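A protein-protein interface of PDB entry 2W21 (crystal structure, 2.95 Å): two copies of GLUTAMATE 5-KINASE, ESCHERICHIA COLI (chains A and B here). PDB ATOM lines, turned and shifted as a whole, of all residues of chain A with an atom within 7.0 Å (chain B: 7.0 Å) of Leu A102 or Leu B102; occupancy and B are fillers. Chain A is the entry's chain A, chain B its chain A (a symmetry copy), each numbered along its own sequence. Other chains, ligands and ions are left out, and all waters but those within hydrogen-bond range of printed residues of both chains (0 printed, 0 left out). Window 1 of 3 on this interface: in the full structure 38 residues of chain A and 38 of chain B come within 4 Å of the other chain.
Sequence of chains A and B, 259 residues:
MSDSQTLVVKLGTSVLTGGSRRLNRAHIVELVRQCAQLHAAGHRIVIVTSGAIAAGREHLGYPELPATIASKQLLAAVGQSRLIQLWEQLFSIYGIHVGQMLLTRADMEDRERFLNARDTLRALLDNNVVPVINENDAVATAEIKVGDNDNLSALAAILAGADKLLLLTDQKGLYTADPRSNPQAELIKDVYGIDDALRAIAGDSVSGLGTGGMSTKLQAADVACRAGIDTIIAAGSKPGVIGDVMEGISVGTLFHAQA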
ATOM      1  N   THR A  49      16.483 -30.972 -15.837  1.00  0.00           N
ATOM      2  CA  THR A  49      15.409 -31.653 -16.564  1.00  0.00           C
ATOM      3  C   THR A  49      15.563 -31.548 -18.088  1.00  0.00           C
ATOM      4  O   THR A  49      15.820 -30.468 -18.604  1.00  0.00           O
ATOM      5  CB  THR A  49      14.042 -31.043 -16.147  1.00  0.00           C
ATOM      6  OG1 THR A  49      12.984 -31.762 -16.767  1.00  0.00           O
ATOM      7  CG2 THR A  49      13.924 -29.603 -16.560  1.00  0.00           C
ATOM      8  N   GLN A  80       8.654 -25.980 -22.569  1.00  0.00           N
ATOM      9  CA  GLN A  80       9.224 -25.587 -21.282  1.00  0.00           C
ATOM     10  C   GLN A  80       8.128 -25.016 -20.403  1.00  0.00           C
ATOM     11  O   GLN A  80       8.091 -25.313 -19.216  1.00  0.00           O
ATOM     12  CB  GLN A  80      10.367 -24.579 -21.469  1.00  0.00           C
ATOM     13  CG  GLN A  80      10.983 -23.996 -20.209  1.00  0.00           C
ATOM     14  CD  GLN A  80      11.847 -24.992 -19.482  1.00  0.00           C
ATOM     15  OE1 GLN A  80      12.538 -25.814 -20.116  1.00  0.00           O
ATOM     16  NE2 GLN A  80      11.827 -24.931 -18.133  1.00  0.00           N
ATOM     17  N   GLN A 100      12.762 -21.913 -11.466  1.00  0.00           N
ATOM     18  CA  GLN A 100      13.123 -22.308 -12.795  1.00  0.00           C
ATOM     19  C   GLN A 100      14.335 -21.536 -13.215  1.00  0.00           C
ATOM     20  O   GLN A 100      14.282 -20.294 -13.267  1.00  0.00           O
ATOM     21  CB  GLN A 100      11.980 -22.001 -13.752  1.00  0.00           C
ATOM     22  CG  GLN A 100      12.286 -22.286 -15.220  1.00  0.00           C
ATOM     23  CD  GLN A 100      11.430 -21.430 -16.139  1.00  0.00           C
ATOM     24  OE1 GLN A 100      10.839 -21.926 -17.096  1.00  0.00           O
ATOM     25  NE2 GLN A 100      11.347 -20.138 -15.846  1.00  0.00           N
ATOM     26  N   MET A 101      15.398 -22.273 -13.565  1.00  0.00           N
ATOM     27  CA  MET A 101      16.582 -21.691 -14.239  1.00  0.00           C
ATOM     28  C   MET A 101      16.859 -22.165 -15.664  1.00  0.00           C
ATOM     29  O   MET A 101      17.164 -23.337 -15.898  1.00  0.00           O
ATOM     30  CB  MET A 101      17.814 -21.932 -13.404  1.00  0.00           C
ATOM     31  CG  MET A 101      17.725 -21.243 -12.056  1.00  0.00           C
ATOM     32  SD  MET A 101      19.362 -21.196 -11.325  1.00  0.00           S
ATOM     33  CE  MET A 101      19.949 -19.624 -11.983  1.00  0.00           C
ATOM     34  N   LEU A 102      16.781 -21.251 -16.618  1.00  0.00           N
ATOM     35  CA  LEU A 102      17.142 -21.597 -17.984  1.00  0.00           C
ATOM     36  C   LEU A 102      18.519 -21.039 -18.342  1.00  0.00           C
ATOM     37  O   LEU A 102      18.698 -19.826 -18.367  1.00  0.00           O
ATOM     38  CB  LEU A 102      16.070 -21.087 -18.938  1.00  0.00           C
ATOM     39  CG  LEU A 102      14.715 -21.717 -18.648  1.00  0.00           C
ATOM     40  CD1 LEU A 102      13.608 -21.079 -19.415  1.00  0.00           C
ATOM     41  CD2 LEU A 102      14.812 -23.162 -19.013  1.00  0.00           C
ATOM     42  N   LEU A 103      19.492 -21.906 -18.623  1.00  0.00           N
ATOM     43  CA  LEU A 103      20.875 -21.455 -18.905  1.00  0.00           C
ATOM     44  C   LEU A 103      21.345 -21.837 -20.295  1.00  0.00           C
ATOM     45  O   LEU A 103      21.061 -22.934 -20.750  1.00  0.00           O
ATOM     46  CB  LEU A 103      21.852 -22.056 -17.888  1.00  0.00           C
ATOM     47  CG  LEU A 103      21.571 -21.873 -16.391  1.00  0.00           C
ATOM     48  CD1 LEU A 103      22.359 -22.837 -15.525  1.00  0.00           C
ATOM     49  CD2 LEU A 103      21.846 -20.440 -15.990  1.00  0.00           C
ATOM     50  N   THR A 104      22.059 -20.943 -20.974  1.00  0.00           N
ATOM     51  CA  THR A 104      22.705 -21.305 -22.256  1.00  0.00           C
ATOM     52  C   THR A 104      24.160 -21.739 -22.052  1.00  0.00           C
ATOM     53  O   THR A 104      24.807 -21.331 -21.078  1.00  0.00           O
ATOM     54  CB  THR A 104      22.680 -20.185 -23.312  1.00  0.00           C
ATOM     55  OG1 THR A 104      23.617 -19.165 -22.965  1.00  0.00           O
ATOM     56  CG2 THR A 104      21.315 -19.561 -23.444  1.00  0.00           C
ATOM     57  N   ASP A 107      26.089 -18.431 -21.619  1.00  0.00           N
ATOM     58  CA  ASP A 107      25.989 -18.013 -20.201  1.00  0.00           C
ATOM     59  C   ASP A 107      27.010 -18.649 -19.250  1.00  0.00           C
ATOM     60  O   ASP A 107      27.339 -18.070 -18.257  1.00  0.00           O
ATOM     61  CB  ASP A 107      24.572 -18.276 -19.636  1.00  0.00           C
ATOM     62  CG  ASP A 107      23.472 -17.492 -20.378  1.00  0.00           C
ATOM     63  OD1 ASP A 107      22.257 -17.803 -20.190  1.00  0.00           O
ATOM     64  OD2 ASP A 107      23.823 -16.570 -21.165  1.00  0.00           O
ATOM     65  N   VAL A 132      15.196 -26.134 -10.816  1.00  0.00           N
ATOM     66  CA  VAL A 132      14.867 -27.032 -11.904  1.00  0.00           C
ATOM     67  C   VAL A 132      15.512 -26.328 -13.090  1.00  0.00           C
ATOM     68  O   VAL A 132      14.991 -25.330 -13.593  1.00  0.00           O
ATOM     69  CB  VAL A 132      13.311 -27.168 -12.062  1.00  0.00           C
ATOM     70  CG1 VAL A 132      12.941 -27.977 -13.265  1.00  0.00           C
ATOM     71  CG2 VAL A 132      12.711 -27.773 -10.841  1.00  0.00           C
ATOM     72  N   ILE A 133      16.669 -26.817 -13.498  1.00  0.00           N
ATOM     73  CA  ILE A 133      17.448 -26.167 -14.529  1.00  0.00           C
ATOM     74  C   ILE A 133      17.352 -26.863 -15.862  1.00  0.00           C
ATOM     75  O   ILE A 133      17.235 -28.074 -15.953  1.00  0.00           O
ATOM     76  CB  ILE A 133      18.902 -26.244 -14.168  1.00  0.00           C
ATOM     77  CG1 ILE A 133      19.108 -25.852 -12.710  1.00  0.00           C
ATOM     78  CG2 ILE A 133      19.727 -25.376 -15.085  1.00  0.00           C
ATOM     79  CD1 ILE A 133      20.369 -26.468 -12.132  1.00  0.00           C
ATOM     80  N   ASN A 134      17.470 -26.094 -16.916  1.00  0.00           N
ATOM     81  CA  ASN A 134      17.468 -26.659 -18.239  1.00  0.00           C
ATOM     82  C   ASN A 134      18.199 -25.707 -19.176  1.00  0.00           C
ATOM     83  O   ASN A 134      18.284 -24.498 -18.921  1.00  0.00           O
ATOM     84  CB  ASN A 134      16.021 -26.856 -18.683  1.00  0.00           C
ATOM     85  CG  ASN A 134      15.884 -27.671 -19.948  1.00  0.00           C
ATOM     86  OD1 ASN A 134      16.810 -28.356 -20.390  1.00  0.00           O
ATOM     87  ND2 ASN A 134      14.699 -27.617 -20.540  1.00  0.00           N
ATOM     88  N   GLU A 135      18.758 -26.266 -20.240  1.00  0.00           N
ATOM     89  CA  GLU A 135      19.208 -25.521 -21.395  1.00  0.00           C
ATOM     90  C   GLU A 135      18.129 -24.551 -21.787  1.00  0.00           C
ATOM     91  O   GLU A 135      16.970 -24.921 -21.803  1.00  0.00           O
ATOM     92  CB  GLU A 135      19.393 -26.517 -22.542  1.00  0.00           C
ATOM     93  CG  GLU A 135      20.499 -26.149 -23.529  1.00  0.00           C
ATOM     94  CD  GLU A 135      21.788 -25.869 -22.781  1.00  0.00           C
ATOM     95  OE1 GLU A 135      22.284 -24.699 -22.836  1.00  0.00           O
ATOM     96  OE2 GLU A 135      22.274 -26.827 -22.097  1.00  0.00           O
ATOM     97  N   ASN A 136      18.480 -23.320 -22.116  1.00  0.00           N
ATOM     98  CA  ASN A 136      17.448 -22.377 -22.546  1.00  0.00           C
ATOM     99  C   ASN A 136      17.128 -22.523 -24.054  1.00  0.00           C
ATOM    100  O   ASN A 136      17.374 -21.617 -24.843  1.00  0.00           O
ATOM    101  CB  ASN A 136      17.811 -20.937 -22.144  1.00  0.00           C
ATOM    102  CG  ASN A 136      16.697 -19.903 -22.442  1.00  0.00           C
ATOM    103  OD1 ASN A 136      15.552 -20.236 -22.751  1.00  0.00           O
ATOM    104  ND2 ASN A 136      17.050 -18.634 -22.341  1.00  0.00           N
ATOM    105  N   ASP A 137      16.533 -23.656 -24.433  1.00  0.00           N
ATOM    106  CA  ASP A 137      16.337 -24.055 -25.832  1.00  0.00           C
ATOM    107  C   ASP A 137      15.534 -23.105 -26.722  1.00  0.00           C
ATOM    108  O   ASP A 137      15.703 -23.139 -27.931  1.00  0.00           O
ATOM    109  CB  ASP A 137      15.743 -25.464 -25.908  1.00  0.00           C
ATOM    110  CG  ASP A 137      16.596 -26.524 -25.168  1.00  0.00           C
ATOM    111  OD1 ASP A 137      17.817 -26.588 -25.443  1.00  0.00           O
ATOM    112  OD2 ASP A 137      16.039 -27.303 -24.331  1.00  0.00           O
ATOM    113  N   ALA A 138      14.679 -22.251 -26.173  1.00  0.00           N
ATOM    114  CA  ALA A 138      13.936 -21.323 -27.037  1.00  0.00           C
ATOM    115  C   ALA A 138      14.818 -20.161 -27.508  1.00  0.00           C
ATOM    116  O   ALA A 138      14.483 -19.396 -28.423  1.00  0.00           O
ATOM    117  CB  ALA A 138      12.705 -20.814 -26.346  1.00  0.00           C
ATOM    118  N   VAL A 139      15.976 -20.039 -26.893  1.00  0.00           N
ATOM    119  CA  VAL A 139      16.848 -18.928 -27.169  1.00  0.00           C
ATOM    120  C   VAL A 139      18.226 -19.457 -27.655  1.00  0.00           C
ATOM    121  O   VAL A 139      18.878 -18.817 -28.517  1.00  0.00           O
ATOM    122  CB  VAL A 139      16.869 -17.999 -25.920  1.00  0.00           C
ATOM    123  CG1 VAL A 139      18.218 -17.326 -25.711  1.00  0.00           C
ATOM    124  CG2 VAL A 139      15.739 -16.995 -25.995  1.00  0.00           C
ATOM    125  N   LEU A 152      25.744 -29.680 -18.896  1.00  0.00           N
ATOM    126  CA  LEU A 152      25.093 -28.699 -18.037  1.00  0.00           C
ATOM    127  C   LEU A 152      24.900 -29.207 -16.618  1.00  0.00           C
ATOM    128  O   LEU A 152      25.144 -28.479 -15.665  1.00  0.00           O
ATOM    129  CB  LEU A 152      23.745 -28.270 -18.615  1.00  0.00           C
ATOM    130  CG  LEU A 152      22.785 -27.432 -17.785  1.00  0.00           C
ATOM    131  CD1 LEU A 152      23.466 -26.199 -17.313  1.00  0.00           C
ATOM    132  CD2 LEU A 152      21.629 -27.018 -18.662  1.00  0.00           C
ATOM    133  N   THR B  49       5.482  -9.740 -20.387  1.00  0.00           N
ATOM    134  CA  THR B  49       4.942  -9.760 -19.026  1.00  0.00           C
ATOM    135  C   THR B  49       5.977  -9.349 -17.969  1.00  0.00           C
ATOM    136  O   THR B  49       7.103  -9.829 -17.997  1.00  0.00           O
ATOM    137  CB  THR B  49       4.423 -11.189 -18.702  1.00  0.00           C
ATOM    138  OG1 THR B  49       3.803 -11.198 -17.423  1.00  0.00           O
ATOM    139  CG2 THR B  49       5.537 -12.196 -18.680  1.00  0.00           C
ATOM    140  N   GLN B  80       8.817 -16.683 -11.888  1.00  0.00           N
ATOM    141  CA  GLN B  80       8.596 -16.924 -13.313  1.00  0.00           C
ATOM    142  C   GLN B  80       7.914 -18.267 -13.493  1.00  0.00           C
ATOM    143  O   GLN B  80       7.009 -18.378 -14.311  1.00  0.00           O
ATOM    144  CB  GLN B  80       9.917 -16.863 -14.094  1.00  0.00           C
ATOM    145  CG  GLN B  80       9.858 -17.204 -15.573  1.00  0.00           C
ATOM    146  CD  GLN B  80       9.212 -16.114 -16.385  1.00  0.00           C
ATOM    147  OE1 GLN B  80       9.389 -14.915 -16.093  1.00  0.00           O
ATOM    148  NE2 GLN B  80       8.451 -16.513 -17.428  1.00  0.00           N
ATOM    149  N   GLN B 100       6.958 -19.774 -23.875  1.00  0.00           N
ATOM    150  CA  GLN B 100       7.657 -18.920 -22.963  1.00  0.00           C
ATOM    151  C   GLN B 100       8.995 -18.584 -23.545  1.00  0.00           C
ATOM    152  O   GLN B 100       9.802 -19.499 -23.790  1.00  0.00           O
ATOM    153  CB  GLN B 100       7.856 -19.636 -21.635  1.00  0.00           C
ATOM    154  CG  GLN B 100       8.681 -18.860 -20.612  1.00  0.00           C
ATOM    155  CD  GLN B 100       9.353 -19.796 -19.620  1.00  0.00           C
ATOM    156  OE1 GLN B 100       9.303 -19.577 -18.412  1.00  0.00           O
ATOM    157  NE2 GLN B 100       9.976 -20.854 -20.125  1.00  0.00           N
ATOM    158  N   MET B 101       9.244 -17.278 -23.711  1.00  0.00           N
ATOM    159  CA  MET B 101      10.594 -16.760 -24.033  1.00  0.00           C
ATOM    160  C   MET B 101      11.257 -15.879 -22.978  1.00  0.00           C
ATOM    161  O   MET B 101      10.787 -14.779 -22.678  1.00  0.00           O
ATOM    162  CB  MET B 101      10.553 -16.003 -25.335  1.00  0.00           C
ATOM    163  CG  MET B 101      10.166 -16.899 -26.496  1.00  0.00           C
ATOM    164  SD  MET B 101      10.569 -16.060 -28.029  1.00  0.00           S
ATOM    165  CE  MET B 101      12.258 -16.645 -28.266  1.00  0.00           C
ATOM    166  N   LEU B 102      12.369 -16.344 -22.429  1.00  0.00           N
ATOM    167  CA  LEU B 102      13.121 -15.515 -21.501  1.00  0.00           C
ATOM    168  C   LEU B 102      14.366 -14.936 -22.173  1.00  0.00           C
ATOM    169  O   LEU B 102      15.252 -15.686 -22.567  1.00  0.00           O
ATOM    170  CB  LEU B 102      13.484 -16.333 -20.268  1.00  0.00           C
ATOM    171  CG  LEU B 102      12.244 -16.829 -19.538  1.00  0.00           C
ATOM    172  CD1 LEU B 102      12.564 -17.809 -18.462  1.00  0.00           C
ATOM    173  CD2 LEU B 102      11.571 -15.634 -18.947  1.00  0.00           C
ATOM    174  N   LEU B 103      14.446 -13.612 -22.305  1.00  0.00           N
ATOM    175  CA  LEU B 103      15.580 -12.970 -23.013  1.00  0.00           C
ATOM    176  C   LEU B 103      16.376 -12.039 -22.121  1.00  0.00           C
ATOM    177  O   LEU B 103      15.794 -11.317 -21.325  1.00  0.00           O
ATOM    178  CB  LEU B 103      15.074 -12.165 -24.215  1.00  0.00           C
ATOM    179  CG  LEU B 103      14.178 -12.858 -25.250  1.00  0.00           C
ATOM    180  CD1 LEU B 103      13.434 -11.875 -26.133  1.00  0.00           C
ATOM    181  CD2 LEU B 103      15.004 -13.814 -26.083  1.00  0.00           C
ATOM    182  N   THR B 104      17.701 -12.048 -22.242  1.00  0.00           N
ATOM    183  CA  THR B 104      18.533 -11.045 -21.541  1.00  0.00           C
ATOM    184  C   THR B 104      18.846  -9.844 -22.440  1.00  0.00           C
ATOM    185  O   THR B 104      18.857  -9.966 -23.672  1.00  0.00           O
ATOM    186  CB  THR B 104      19.863 -11.598 -20.998  1.00  0.00           C
ATOM    187  OG1 THR B 104      20.778 -11.815 -22.073  1.00  0.00           O
ATOM    188  CG2 THR B 104      19.676 -12.896 -20.256  1.00  0.00           C
ATOM    189  N   ASP B 107      21.675 -11.088 -24.743  1.00  0.00           N
ATOM    190  CA  ASP B 107      21.067 -11.813 -25.882  1.00  0.00           C
ATOM    191  C   ASP B 107      20.598 -10.936 -27.050  1.00  0.00           C
ATOM    192  O   ASP B 107      20.552 -11.393 -28.155  1.00  0.00           O
ATOM    193  CB  ASP B 107      19.872 -12.683 -25.421  1.00  0.00           C
ATOM    194  CG  ASP B 107      20.274 -13.770 -24.405  1.00  0.00           C
ATOM    195  OD1 ASP B 107      19.369 -14.378 -23.760  1.00  0.00           O
ATOM    196  OD2 ASP B 107      21.502 -14.006 -24.238  1.00  0.00           O
ATOM    197  N   VAL B 132       5.040 -15.329 -24.728  1.00  0.00           N
ATOM    198  CA  VAL B 132       4.936 -14.619 -23.470  1.00  0.00           C
ATOM    199  C   VAL B 132       6.401 -14.407 -23.114  1.00  0.00           C
ATOM    200  O   VAL B 132       7.086 -15.334 -22.675  1.00  0.00           O
ATOM    201  CB  VAL B 132       4.178 -15.487 -22.403  1.00  0.00           C
ATOM    202  CG1 VAL B 132       4.179 -14.839 -21.056  1.00  0.00           C
ATOM    203  CG2 VAL B 132       2.780 -15.749 -22.838  1.00  0.00           C
ATOM    204  N   ILE B 133       6.889 -13.205 -23.352  1.00  0.00           N
ATOM    205  CA  ILE B 133       8.295 -12.906 -23.179  1.00  0.00           C
ATOM    206  C   ILE B 133       8.578 -12.129 -21.920  1.00  0.00           C
ATOM    207  O   ILE B 133       7.792 -11.311 -21.474  1.00  0.00           O
ATOM    208  CB  ILE B 133       8.745 -12.004 -24.289  1.00  0.00           C
ATOM    209  CG1 ILE B 133       8.246 -12.522 -25.632  1.00  0.00           C
ATOM    210  CG2 ILE B 133      10.247 -11.862 -24.286  1.00  0.00           C
ATOM    211  CD1 ILE B 133       8.127 -11.411 -26.658  1.00  0.00           C
ATOM    212  N   ASN B 134       9.750 -12.339 -21.373  1.00  0.00           N
ATOM    213  CA  ASN B 134      10.158 -11.597 -20.210  1.00  0.00           C
ATOM    214  C   ASN B 134      11.680 -11.572 -20.158  1.00  0.00           C
ATOM    215  O   ASN B 134      12.353 -12.452 -20.711  1.00  0.00           O
ATOM    216  CB  ASN B 134       9.582 -12.278 -18.971  1.00  0.00           C
ATOM    217  CG  ASN B 134       9.728 -11.459 -17.709  1.00  0.00           C
ATOM    218  OD1 ASN B 134       9.998 -10.255 -17.737  1.00  0.00           O
ATOM    219  ND2 ASN B 134       9.530 -12.113 -16.574  1.00  0.00           N
ATOM    220  N   GLU B 135      12.215 -10.538 -19.524  1.00  0.00           N
ATOM    221  CA  GLU B 135      13.593 -10.490 -19.087  1.00  0.00           C
ATOM    222  C   GLU B 135      13.921 -11.786 -18.399  1.00  0.00           C
ATOM    223  O   GLU B 135      13.123 -12.265 -17.615  1.00  0.00           O
ATOM    224  CB  GLU B 135      13.711  -9.362 -18.059  1.00  0.00           C
ATOM    225  CG  GLU B 135      15.068  -8.661 -18.040  1.00  0.00           C
ATOM    226  CD  GLU B 135      15.442  -8.221 -19.441  1.00  0.00           C
ATOM    227  OE1 GLU B 135      16.474  -8.728 -19.986  1.00  0.00           O
ATOM    228  OE2 GLU B 135      14.660  -7.390 -20.010  1.00  0.00           O
ATOM    229  N   ASN B 136      15.081 -12.361 -18.665  1.00  0.00           N
ATOM    230  CA  ASN B 136      15.437 -13.597 -17.969  1.00  0.00           C
ATOM    231  C   ASN B 136      16.068 -13.316 -16.584  1.00  0.00           C
ATOM    232  O   ASN B 136      17.236 -13.609 -16.350  1.00  0.00           O
ATOM    233  CB  ASN B 136      16.310 -14.501 -18.857  1.00  0.00           C
ATOM    234  CG  ASN B 136      16.608 -15.889 -18.238  1.00  0.00           C
ATOM    235  OD1 ASN B 136      16.013 -16.311 -17.245  1.00  0.00           O
ATOM    236  ND2 ASN B 136      17.541 -16.600 -18.844  1.00  0.00           N
ATOM    237  N   ASP B 137      15.267 -12.790 -15.655  1.00  0.00           N
ATOM    238  CA  ASP B 137      15.732 -12.273 -14.362  1.00  0.00           C
ATOM    239  C   ASP B 137      16.474 -13.250 -13.449  1.00  0.00           C
ATOM    240  O   ASP B 137      17.242 -12.809 -12.608  1.00  0.00           O
ATOM    241  CB  ASP B 137      14.574 -11.625 -13.598  1.00  0.00           C
ATOM    242  CG  ASP B 137      13.875 -10.498 -14.398  1.00  0.00           C
ATOM    243  OD1 ASP B 137      14.592  -9.593 -14.885  1.00  0.00           O
ATOM    244  OD2 ASP B 137      12.608 -10.510 -14.518  1.00  0.00           O
ATOM    245  N   ALA B 138      16.285 -14.556 -13.588  1.00  0.00           N
ATOM    246  CA  ALA B 138      17.028 -15.485 -12.723  1.00  0.00           C
ATOM    247  C   ALA B 138      18.487 -15.631 -13.172  1.00  0.00           C
ATOM    248  O   ALA B 138      19.352 -16.167 -12.466  1.00  0.00           O
ATOM    249  CB  ALA B 138      16.349 -16.823 -12.663  1.00  0.00           C
ATOM    250  N   VAL B 139      18.772 -15.127 -14.354  1.00  0.00           N
ATOM    251  CA  VAL B 139      20.078 -15.293 -14.934  1.00  0.00           C
ATOM    252  C   VAL B 139      20.696 -13.898 -15.232  1.00  0.00           C
ATOM    253  O   VAL B 139      21.933 -13.718 -15.112  1.00  0.00           O
ATOM    254  CB  VAL B 139      19.958 -16.265 -16.144  1.00  0.00           C
ATOM    255  CG1 VAL B 139      20.931 -15.930 -17.266  1.00  0.00           C
ATOM    256  CG2 VAL B 139      20.098 -17.698 -15.679  1.00  0.00           C
ATOM    257  N   LEU B 152      12.642  -3.908 -23.781  1.00  0.00           N
ATOM    258  CA  LEU B 152      12.454  -5.253 -24.310  1.00  0.00           C
ATOM    259  C   LEU B 152      11.201  -5.372 -25.160  1.00  0.00           C
ATOM    260  O   LEU B 152      11.233  -5.980 -26.222  1.00  0.00           O
ATOM    261  CB  LEU B 152      12.409  -6.286 -23.185  1.00  0.00           C
ATOM    262  CG  LEU B 152      11.996  -7.720 -23.475  1.00  0.00           C
ATOM    263  CD1 LEU B 152      12.849  -8.287 -24.549  1.00  0.00           C
ATOM    264  CD2 LEU B 152      12.211  -8.542 -22.228  1.00  0.00           C
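Gln A80 touches Gln B100, and with the chains exchanged Gln A100 touches Gln B80.
Met A101 touches Ala B138, and with the chains exchanged Ala A138 touches Met B101.
Leu B102 touches its own counterpart, Leu A102.
Asp A107 touches Val B139, and with the chains exchanged Val A139 touches Asp B107.
The side-chain amide oxygen (OE1) of Gln A100 lies close to the side-chain amide oxygen (OE1) of Gln B100, 3.1 Å away.
ND2 of Asn B136 is in hydrogen-bond range of O of Leu A102, 3.5 Å away.
The backbone carbonyl oxygen (O) of Leu B102 is in hydrogen-bond range of the side-chain amide nitrogen (ND2) of Asn A136 (3.5 Å).
Printed residues of chain A that touch a printed residue of chain B: Gln A80, Gln A100, Met A101, Leu A102, Leu A103, Asp A107, Asn A136, Ala A138 and Val A139.
Hydrophobic or aromatic side chains of chain A within 4 Å of the printed part of chain B: Met A101, Leu A102, Leu A103 and Val A139.
Among the printed residues, no Asp or Glu carboxylate lies within 4 Å of a Lys or Arg side-chain nitrogen of the other chain.
NE2 of Gln A100 touches CG of Gln B80, 3.3 Å away.
NE2 of Gln A100 touches CD1 of Leu B102 (3.7 Å).
Met A101 touches Ala B138 (CE to O, 3.5 Å).
Gln B100 touches Leu A102 (NE2 to CD1, 3.7 Å).
Leu A102 touches Val B139 (O to CG2, 3.7 Å).
Leu A103 touches Val B139 (CD2 to CG2, 3.3 Å).
Asp A107 touches Val B139.
Ala A138 touches Met B101 (O to CE, 3.5 Å).
Val A139 touches Leu B102 (CG2 to O, 3.7 Å).
Val A139 touches Leu B103.
O of Met A101 lies within hydrogen-bond range of N of Asn A134 (3.0 Å).
The backbone NH (N) of Leu A103 sits at hydrogen-bond distance from the backbone carbonyl oxygen (O) of Asn A134 (2.9 Å).
OE1 of Gln B80 lies within hydrogen-bond range of ND2 of Asn B134, at 2.8 Å.
The backbone carbonyl oxygen of Val B132 is in hydrogen-bond range of the backbone NH of Met B101, at 3.1 Å.
N of Leu B103 lies within hydrogen-bond range of O of Asn B134 (2.9 Å).
The backbone NH (N) of Asp B107 is in hydrogen-bond range of the side-chain hydroxyl (OG1) of Thr B104 (2.9 Å).
Printed residues of chain B within 4 Å of Gln A80: Gln B100 (3.3 Å).
Of chain B, only Gln B100 (3.7 Å), Leu B102 (3.6 Å), Asn B136 (3.5 Å) and Val B139 (3.7 Å) come within 4 Å of Leu A102.
Val A132 touches none of the printed residues of chain B.
Printed residues of chain A within 4 Å of Gln B100: Gln A80 (3.3 Å), Gln A100 (3.1 Å) and Leu A102 (3.7 Å).
Of chain A, only Gln A100 (3.7 Å), Leu A102 (3.6 Å), Asn A136 (3.5 Å) and Val A139 (3.7 Å) come within 4 Å of Leu B102.
Asn B134 touches none of the printed residues of chain A.
The nearest residue of chain B that does not touch Leu A102 is Ala B138 (6.0 Å).
The nearest residue of chain A that does not touch Leu B102 is Ala A138 (6.0 Å).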
